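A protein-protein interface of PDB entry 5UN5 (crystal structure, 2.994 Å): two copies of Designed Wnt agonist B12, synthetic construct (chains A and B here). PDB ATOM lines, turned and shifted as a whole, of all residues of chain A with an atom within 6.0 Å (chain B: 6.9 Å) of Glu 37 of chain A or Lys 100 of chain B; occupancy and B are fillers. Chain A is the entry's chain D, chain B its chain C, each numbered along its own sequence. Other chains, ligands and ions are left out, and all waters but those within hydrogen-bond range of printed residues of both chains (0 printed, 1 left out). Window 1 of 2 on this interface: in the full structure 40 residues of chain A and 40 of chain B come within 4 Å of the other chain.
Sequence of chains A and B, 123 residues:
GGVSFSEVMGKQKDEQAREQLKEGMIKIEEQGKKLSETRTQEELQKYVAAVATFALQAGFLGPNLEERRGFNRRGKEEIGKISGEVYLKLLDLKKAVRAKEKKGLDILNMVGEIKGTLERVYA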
ATOM      1  N   GLY A  32      29.097  -6.719 -13.485  1.00  0.00           N
ATOM      2  CA  GLY A  32      27.744  -6.852 -12.977  1.00  0.00           C
ATOM      3  C   GLY A  32      27.548  -8.081 -12.115  1.00  0.00           C
ATOM      4  O   GLY A  32      26.763  -8.055 -11.163  1.00  0.00           O
ATOM      5  N   LYS A  33      28.254  -9.170 -12.434  1.00  0.00           N
ATOM      6  CA  LYS A  33      28.120 -10.405 -11.667  1.00  0.00           C
ATOM      7  C   LYS A  33      28.592 -10.223 -10.230  1.00  0.00           C
ATOM      8  O   LYS A  33      27.920 -10.653  -9.285  1.00  0.00           O
ATOM      9  CB  LYS A  33      28.899 -11.528 -12.355  1.00  0.00           C
ATOM     10  CG  LYS A  33      28.681 -12.906 -11.752  1.00  0.00           C
ATOM     11  CD  LYS A  33      29.373 -13.978 -12.580  1.00  0.00           C
ATOM     12  CE  LYS A  33      29.088 -15.370 -12.038  1.00  0.00           C
ATOM     13  NZ  LYS A  33      29.607 -15.546 -10.652  1.00  0.00           N
ATOM     14  N   LYS A  34      29.750  -9.584 -10.041  1.00  0.00           N
ATOM     15  CA  LYS A  34      30.250  -9.375  -8.686  1.00  0.00           C
ATOM     16  C   LYS A  34      29.446  -8.310  -7.950  1.00  0.00           C
ATOM     17  O   LYS A  34      29.353  -8.346  -6.719  1.00  0.00           O
ATOM     18  CB  LYS A  34      31.734  -9.008  -8.711  1.00  0.00           C
ATOM     19  CG  LYS A  34      32.072  -7.759  -9.502  1.00  0.00           C
ATOM     20  CD  LYS A  34      33.569  -7.487  -9.472  1.00  0.00           C
ATOM     21  CE  LYS A  34      34.357  -8.665 -10.029  1.00  0.00           C
ATOM     22  NZ  LYS A  34      35.826  -8.433  -9.968  1.00  0.00           N
ATOM     23  N   LEU A  35      28.869  -7.356  -8.683  1.00  0.00           N
ATOM     24  CA  LEU A  35      28.017  -6.351  -8.054  1.00  0.00           C
ATOM     25  C   LEU A  35      26.739  -6.981  -7.515  1.00  0.00           C
ATOM     26  O   LEU A  35      26.336  -6.724  -6.375  1.00  0.00           O
ATOM     27  CB  LEU A  35      27.694  -5.244  -9.059  1.00  0.00           C
ATOM     28  CG  LEU A  35      26.681  -4.182  -8.637  1.00  0.00           C
ATOM     29  CD1 LEU A  35      27.105  -3.515  -7.339  1.00  0.00           C
ATOM     30  CD2 LEU A  35      26.514  -3.154  -9.745  1.00  0.00           C
ATOM     31  N   SER A  36      26.089  -7.815  -8.327  1.00  0.00           N
ATOM     32  CA  SER A  36      24.847  -8.466  -7.936  1.00  0.00           C
ATOM     33  C   SER A  36      25.060  -9.622  -6.969  1.00  0.00           C
ATOM     34  O   SER A  36      24.095 -10.058  -6.333  1.00  0.00           O
ATOM     35  CB  SER A  36      24.101  -8.954  -9.177  1.00  0.00           C
ATOM     36  OG  SER A  36      24.962  -9.008 -10.298  1.00  0.00           O
ATOM     37  N   GLU A  37      26.284 -10.139  -6.862  1.00  0.00           N
ATOM     38  CA  GLU A  37      26.555 -11.265  -5.976  1.00  0.00           C
ATOM     39  C   GLU A  37      26.230 -10.907  -4.531  1.00  0.00           C
ATOM     40  O   GLU A  37      26.645  -9.860  -4.027  1.00  0.00           O
ATOM     41  CB  GLU A  37      28.020 -11.691  -6.093  1.00  0.00           C
ATOM     42  CG  GLU A  37      28.512 -12.535  -4.920  1.00  0.00           C
ATOM     43  CD  GLU A  37      29.803 -13.279  -5.219  1.00  0.00           C
ATOM     44  OE1 GLU A  37      30.869 -12.848  -4.729  1.00  0.00           O
ATOM     45  OE2 GLU A  37      29.750 -14.296  -5.940  1.00  0.00           O
ATOM     46  N   THR A  38      25.483 -11.786  -3.865  1.00  0.00           N
ATOM     47  CA  THR A  38      25.090 -11.557  -2.482  1.00  0.00           C
ATOM     48  C   THR A  38      25.853 -12.487  -1.546  1.00  0.00           C
ATOM     49  O   THR A  38      26.809 -12.057  -0.890  1.00  0.00           O
ATOM     50  CB  THR A  38      23.581 -11.757  -2.313  1.00  0.00           C
ATOM     51  OG1 THR A  38      23.223 -13.069  -2.762  1.00  0.00           O
ATOM     52  CG2 THR A  38      22.814 -10.723  -3.123  1.00  0.00           C
ATOM     53  N   ARG A  39      25.433 -13.752  -1.469  1.00  0.00           N
ATOM     54  CA  ARG A  39      26.156 -14.786  -0.724  1.00  0.00           C
ATOM     55  C   ARG A  39      26.231 -14.461   0.766  1.00  0.00           C
ATOM     56  O   ARG A  39      27.150 -14.896   1.466  1.00  0.00           O
ATOM     57  CB  ARG A  39      27.562 -15.007  -1.293  1.00  0.00           C
ATOM     58  CG  ARG A  39      27.587 -15.532  -2.723  1.00  0.00           C
ATOM     59  CD  ARG A  39      27.100 -16.970  -2.800  1.00  0.00           C
ATOM     60  NE  ARG A  39      27.281 -17.536  -4.135  1.00  0.00           N
ATOM     61  CZ  ARG A  39      27.099 -18.817  -4.435  1.00  0.00           C
ATOM     62  NH1 ARG A  39      26.729 -19.675  -3.495  1.00  0.00           N
ATOM     63  NH2 ARG A  39      27.289 -19.243  -5.678  1.00  0.00           N
ATOM     64  N   THR A  40      25.262 -13.688   1.259  1.00  0.00           N
ATOM     65  CA  THR A  40      25.295 -13.233   2.645  1.00  0.00           C
ATOM     66  C   THR A  40      24.982 -14.364   3.617  1.00  0.00           C
ATOM     67  O   THR A  40      25.548 -14.418   4.715  1.00  0.00           O
ATOM     68  CB  THR A  40      24.323 -12.069   2.837  1.00  0.00           C
ATOM     69  OG1 THR A  40      24.567 -11.076   1.832  1.00  0.00           O
ATOM     70  CG2 THR A  40      24.517 -11.436   4.204  1.00  0.00           C
ATOM     71  N   LYS A 100      18.753  -7.513   3.361  1.00  0.00           N
ATOM     72  CA  LYS A 100      19.912  -7.205   2.531  1.00  0.00           C
ATOM     73  C   LYS A 100      19.977  -8.137   1.325  1.00  0.00           C
ATOM     74  O   LYS A 100      20.372  -7.720   0.230  1.00  0.00           O
ATOM     75  CB  LYS A 100      21.194  -7.303   3.360  1.00  0.00           C
ATOM     76  CG  LYS A 100      22.465  -7.028   2.570  1.00  0.00           C
ATOM     77  CD  LYS A 100      23.699  -7.073   3.455  1.00  0.00           C
ATOM     78  CE  LYS A 100      24.967  -6.828   2.649  1.00  0.00           C
ATOM     79  NZ  LYS A 100      26.193  -6.908   3.492  1.00  0.00           N
ATOM     80  N   LYS A 103      17.465  -6.710  -1.278  1.00  0.00           N
ATOM     81  CA  LYS A 103      18.002  -5.587  -2.038  1.00  0.00           C
ATOM     82  C   LYS A 103      19.077  -6.054  -3.010  1.00  0.00           C
ATOM     83  O   LYS A 103      19.174  -5.544  -4.132  1.00  0.00           O
ATOM     84  CB  LYS A 103      18.554  -4.520  -1.093  1.00  0.00           C
ATOM     85  CG  LYS A 103      17.511  -3.910  -0.167  1.00  0.00           C
ATOM     86  CD  LYS A 103      16.339  -3.328  -0.945  1.00  0.00           C
ATOM     87  CE  LYS A 103      16.782  -2.245  -1.916  1.00  0.00           C
ATOM     88  NZ  LYS A 103      15.643  -1.729  -2.724  1.00  0.00           N
ATOM     89  N   GLY A 104      19.898  -7.022  -2.593  1.00  0.00           N
ATOM     90  CA  GLY A 104      20.866  -7.604  -3.505  1.00  0.00           C
ATOM     91  C   GLY A 104      20.212  -8.280  -4.693  1.00  0.00           C
ATOM     92  O   GLY A 104      20.754  -8.265  -5.801  1.00  0.00           O
ATOM     93  N   ILE A 107      19.157  -5.651  -7.148  1.00  0.00           N
ATOM     94  CA  ILE A 107      20.318  -5.238  -7.931  1.00  0.00           C
ATOM     95  C   ILE A 107      20.573  -6.227  -9.062  1.00  0.00           C
ATOM     96  O   ILE A 107      20.950  -5.838 -10.175  1.00  0.00           O
ATOM     97  CB  ILE A 107      21.547  -5.085  -7.016  1.00  0.00           C
ATOM     98  CG1 ILE A 107      21.305  -3.981  -5.984  1.00  0.00           C
ATOM     99  CG2 ILE A 107      22.795  -4.786  -7.831  1.00  0.00           C
ATOM    100  CD1 ILE A 107      22.476  -3.730  -5.064  1.00  0.00           C
ATOM    101  N   THR B  38      29.901  -5.229   3.639  1.00  0.00           N
ATOM    102  CA  THR B  38      29.002  -5.017   2.512  1.00  0.00           C
ATOM    103  C   THR B  38      29.796  -4.716   1.241  1.00  0.00           C
ATOM    104  O   THR B  38      29.887  -5.577   0.358  1.00  0.00           O
ATOM    105  CB  THR B  38      27.966  -3.934   2.848  1.00  0.00           C
ATOM    106  OG1 THR B  38      27.311  -3.493   1.652  1.00  0.00           O
ATOM    107  CG2 THR B  38      28.593  -2.757   3.588  1.00  0.00           C
ATOM    108  N   THR B  40      29.261  -2.943  -1.365  1.00  0.00           N
ATOM    109  CA  THR B  40      28.542  -3.014  -2.631  1.00  0.00           C
ATOM    110  C   THR B  40      28.852  -1.811  -3.512  1.00  0.00           C
ATOM    111  O   THR B  40      28.991  -1.949  -4.732  1.00  0.00           O
ATOM    112  CB  THR B  40      27.039  -3.115  -2.371  1.00  0.00           C
ATOM    113  OG1 THR B  40      26.781  -4.183  -1.450  1.00  0.00           O
ATOM    114  CG2 THR B  40      26.290  -3.377  -3.669  1.00  0.00           C
ATOM    115  N   GLU B  43      32.114  -1.894  -5.533  1.00  0.00           N
ATOM    116  CA  GLU B  43      31.959  -2.700  -6.740  1.00  0.00           C
ATOM    117  C   GLU B  43      31.130  -1.982  -7.796  1.00  0.00           C
ATOM    118  O   GLU B  43      31.279  -2.258  -8.992  1.00  0.00           O
ATOM    119  CB  GLU B  43      31.326  -4.047  -6.392  1.00  0.00           C
ATOM    120  CG  GLU B  43      32.192  -4.919  -5.498  1.00  0.00           C
ATOM    121  CD  GLU B  43      31.426  -6.080  -4.898  1.00  0.00           C
ATOM    122  OE1 GLU B  43      30.180  -6.082  -4.988  1.00  0.00           O
ATOM    123  OE2 GLU B  43      32.070  -6.987  -4.329  1.00  0.00           O
ATOM    124  N   LYS B  95      20.589   3.924  -6.547  1.00  0.00           N
ATOM    125  CA  LYS B  95      19.714   4.001  -5.382  1.00  0.00           C
ATOM    126  C   LYS B  95      19.654   2.661  -4.658  1.00  0.00           C
ATOM    127  O   LYS B  95      19.761   2.601  -3.428  1.00  0.00           O
ATOM    128  CB  LYS B  95      18.316   4.454  -5.804  1.00  0.00           C
ATOM    129  CG  LYS B  95      18.243   5.912  -6.220  1.00  0.00           C
ATOM    130  CD  LYS B  95      16.839   6.299  -6.654  1.00  0.00           C
ATOM    131  CE  LYS B  95      16.803   7.723  -7.190  1.00  0.00           C
ATOM    132  NZ  LYS B  95      15.521   8.026  -7.886  1.00  0.00           N
ATOM    133  N   ALA B  96      19.467   1.573  -5.413  1.00  0.00           N
ATOM    134  CA  ALA B  96      19.396   0.248  -4.804  1.00  0.00           C
ATOM    135  C   ALA B  96      20.705  -0.119  -4.117  1.00  0.00           C
ATOM    136  O   ALA B  96      20.699  -0.742  -3.048  1.00  0.00           O
ATOM    137  CB  ALA B  96      19.034  -0.795  -5.863  1.00  0.00           C
ATOM    138  N   VAL B  97      21.838   0.250  -4.718  1.00  0.00           N
ATOM    139  CA  VAL B  97      23.131  -0.008  -4.090  1.00  0.00           C
ATOM    140  C   VAL B  97      23.236   0.752  -2.775  1.00  0.00           C
ATOM    141  O   VAL B  97      23.650   0.203  -1.746  1.00  0.00           O
ATOM    142  CB  VAL B  97      24.279   0.355  -5.050  1.00  0.00           C
ATOM    143  CG1 VAL B  97      25.615   0.261  -4.335  1.00  0.00           C
ATOM    144  CG2 VAL B  97      24.263  -0.558  -6.263  1.00  0.00           C
ATOM    145  N   ARG B  98      22.856   2.033  -2.790  1.00  0.00           N
ATOM    146  CA  ARG B  98      22.844   2.820  -1.561  1.00  0.00           C
ATOM    147  C   ARG B  98      21.859   2.252  -0.548  1.00  0.00           C
ATOM    148  O   ARG B  98      22.092   2.340   0.663  1.00  0.00           O
ATOM    149  CB  ARG B  98      22.507   4.276  -1.887  1.00  0.00           C
ATOM    150  CG  ARG B  98      22.592   5.227  -0.707  1.00  0.00           C
ATOM    151  CD  ARG B  98      22.407   6.678  -1.143  1.00  0.00           C
ATOM    152  NE  ARG B  98      21.098   6.923  -1.743  1.00  0.00           N
ATOM    153  CZ  ARG B  98      20.879   7.037  -3.051  1.00  0.00           C
ATOM    154  NH1 ARG B  98      21.885   6.936  -3.909  1.00  0.00           N
ATOM    155  NH2 ARG B  98      19.651   7.260  -3.502  1.00  0.00           N
ATOM    156  N   ALA B  99      20.756   1.667  -1.019  1.00  0.00           N
ATOM    157  CA  ALA B  99      19.817   1.009  -0.117  1.00  0.00           C
ATOM    158  C   ALA B  99      20.417  -0.261   0.476  1.00  0.00           C
ATOM    159  O   ALA B  99      20.297  -0.513   1.681  1.00  0.00           O
ATOM    160  CB  ALA B  99      18.514   0.698  -0.853  1.00  0.00           C
ATOM    161  N   LYS B 100      21.063  -1.079  -0.360  1.00  0.00           N
ATOM    162  CA  LYS B 100      21.721  -2.282   0.143  1.00  0.00           C
ATOM    163  C   LYS B 100      22.859  -1.930   1.093  1.00  0.00           C
ATOM    164  O   LYS B 100      23.098  -2.640   2.077  1.00  0.00           O
ATOM    165  CB  LYS B 100      22.231  -3.130  -1.021  1.00  0.00           C
ATOM    166  CG  LYS B 100      22.956  -4.402  -0.597  1.00  0.00           C
ATOM    167  CD  LYS B 100      23.375  -5.232  -1.797  1.00  0.00           C
ATOM    168  CE  LYS B 100      24.122  -6.484  -1.368  1.00  0.00           C
ATOM    169  NZ  LYS B 100      24.573  -7.290  -2.536  1.00  0.00           N
ATOM    170  N   GLU B 101      23.570  -0.835   0.816  1.00  0.00           N
ATOM    171  CA  GLU B 101      24.616  -0.383   1.725  1.00  0.00           C
ATOM    172  C   GLU B 101      24.043  -0.012   3.087  1.00  0.00           C
ATOM    173  O   GLU B 101      24.690  -0.238   4.116  1.00  0.00           O
ATOM    174  CB  GLU B 101      25.358   0.808   1.115  1.00  0.00           C
ATOM    175  CG  GLU B 101      26.628   1.213   1.849  1.00  0.00           C
ATOM    176  CD  GLU B 101      27.844   0.428   1.392  1.00  0.00           C
ATOM    177  OE1 GLU B 101      27.761  -0.245   0.343  1.00  0.00           O
ATOM    178  OE2 GLU B 101      28.885   0.487   2.081  1.00  0.00           O
ATOM    179  N   LYS B 102      22.830   0.545   3.115  1.00  0.00           N
ATOM    180  CA  LYS B 102      22.208   0.934   4.377  1.00  0.00           C
ATOM    181  C   LYS B 102      21.843  -0.283   5.218  1.00  0.00           C
ATOM    182  O   LYS B 102      22.018  -0.274   6.442  1.00  0.00           O
ATOM    183  CB  LYS B 102      20.973   1.793   4.108  1.00  0.00           C
ATOM    184  CG  LYS B 102      20.321   2.342   5.362  1.00  0.00           C
ATOM    185  CD  LYS B 102      19.102   3.184   5.031  1.00  0.00           C
ATOM    186  CE  LYS B 102      18.502   3.791   6.290  1.00  0.00           C
ATOM    187  NZ  LYS B 102      19.464   4.695   6.981  1.00  0.00           N
ATOM    188  N   LYS B 103      21.320  -1.335   4.581  1.00  0.00           N
ATOM    189  CA  LYS B 103      20.991  -2.558   5.307  1.00  0.00           C
ATOM    190  C   LYS B 103      22.233  -3.196   5.915  1.00  0.00           C
ATOM    191  O   LYS B 103      22.170  -3.780   7.003  1.00  0.00           O
ATOM    192  CB  LYS B 103      20.283  -3.546   4.378  1.00  0.00           C
ATOM    193  CG  LYS B 103      18.951  -3.053   3.842  1.00  0.00           C
ATOM    194  CD  LYS B 103      18.008  -2.686   4.974  1.00  0.00           C
ATOM    195  CE  LYS B 103      16.662  -2.219   4.446  1.00  0.00           C
ATOM    196  NZ  LYS B 103      15.722  -1.882   5.552  1.00  0.00           N
ATOM    197  N   GLY B 104      23.373  -3.100   5.225  1.00  0.00           N
ATOM    198  CA  GLY B 104      24.610  -3.624   5.778  1.00  0.00           C
ATOM    199  C   GLY B 104      24.988  -2.997   7.103  1.00  0.00           C
ATOM    200  O   GLY B 104      25.561  -3.666   7.968  1.00  0.00           O
ATOM    201  N   LEU B 105      24.679  -1.711   7.285  1.00  0.00           N
ATOM    202  CA  LEU B 105      24.938  -1.068   8.571  1.00  0.00           C
ATOM    203  C   LEU B 105      23.993  -1.584   9.648  1.00  0.00           C
ATOM    204  O   LEU B 105      24.394  -1.743  10.807  1.00  0.00           O
ATOM    205  CB  LEU B 105      24.829   0.452   8.443  1.00  0.00           C
ATOM    206  CG  LEU B 105      26.036   1.245   7.931  1.00  0.00           C
ATOM    207  CD1 LEU B 105      26.465   0.826   6.530  1.00  0.00           C
ATOM    208  CD2 LEU B 105      25.738   2.737   7.977  1.00  0.00           C
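Of the 13 printed residues of chain A, 8 touch a printed residue of chain B. Hydrophobic or aromatic side chains of chain A within 4 Å of the printed part of chain B: Leu 35 and Ile 107. Along chain A the printed residues that touch a printed residue of chain B span positions 34 to 107. Of the 14 printed residues of chain B, 8 touch a printed residue of chain A. Along chain B the printed residues that touch a printed residue of chain A span positions 38 to 103.
Thr 38 of chain A touches Lys 100 of chain B, and with the chains exchanged Lys 100 of chain A touches Thr 38 of chain B. Lys 100 of chain A touches Lys 103 of chain B, and with the chains exchanged Lys 103 of chain A touches Lys 100 of chain B. Gly 104 of chain A touches Lys 100 of chain B, but with the chains exchanged Lys 100 of chain A does not touch Gly 104 of chain B (4.3 Å). Of the 13 pairs that touch across the chains among the printed residues, 4 have their exchanged pair printed and touching as well.
Among the printed residues, pairs that only touch across the chains: Lys 100 of chain A with Thr 38 of chain B (3.5 Å), Lys 103 of chain A with Ala 99 of chain B (3.6 Å), Leu 35 of chain A with Thr 40 of chain B (3.6 Å), Glu 37 of chain A with Lys 100 of chain B (3.6 Å), Ile 107 of chain A with Lys 100 of chain B (3.7 Å), Leu 35 of chain A with Glu 43 of chain B (3.8 Å), Ile 107 of chain A with Val 97 of chain B (3.8 Å), Gly 104 of chain A with Lys 100 of chain B (3.8 Å), Thr 38 of chain A with Lys 100 of chain B (3.9 Å), Ile 107 of chain A with Ala 96 of chain B (3.9 Å), Lys 103 of chain A with Lys 100 of chain B (3.9 Å) and Lys 100 of chain A with Lys 103 of chain B (3.998 Å).
The side-chain carboxylate of Glu 43 of chain B lies close to the backbone carbonyl oxygen of Lys 34 of chain A (3.0 Å).
Of the printed residues of chain B, Leu 35 of chain A touches Thr 40 and Glu 43. Glu 37 of chain A touches just one residue of chain B: Lys 100. Of the printed residues of chain B, Lys 100 of chain A touches Thr 38 and Lys 103. Of the printed residues of chain B, Ile 107 of chain A touches Ala 96, Val 97 and Lys 100. Printed residues of chain A within 4 Å of Thr 40 of chain B: Leu 35 (3.6 Å). Lys 100 of chain B touches five residues of chain A. The nearest residue of chain A that does not touch Lys 100 of chain B is Lys 100 of chain A (4.1 Å). The nearest printed residue of chain A that does not touch Ala 96 of chain B is Lys 103 of chain A (4.3 Å).
The side-chain hydroxyl (OG1) of Thr 38 of chain B is in hydrogen-bond range of the side-chain hydroxyl (OG1) of Thr 40 of chain B, at 3.2 Å.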
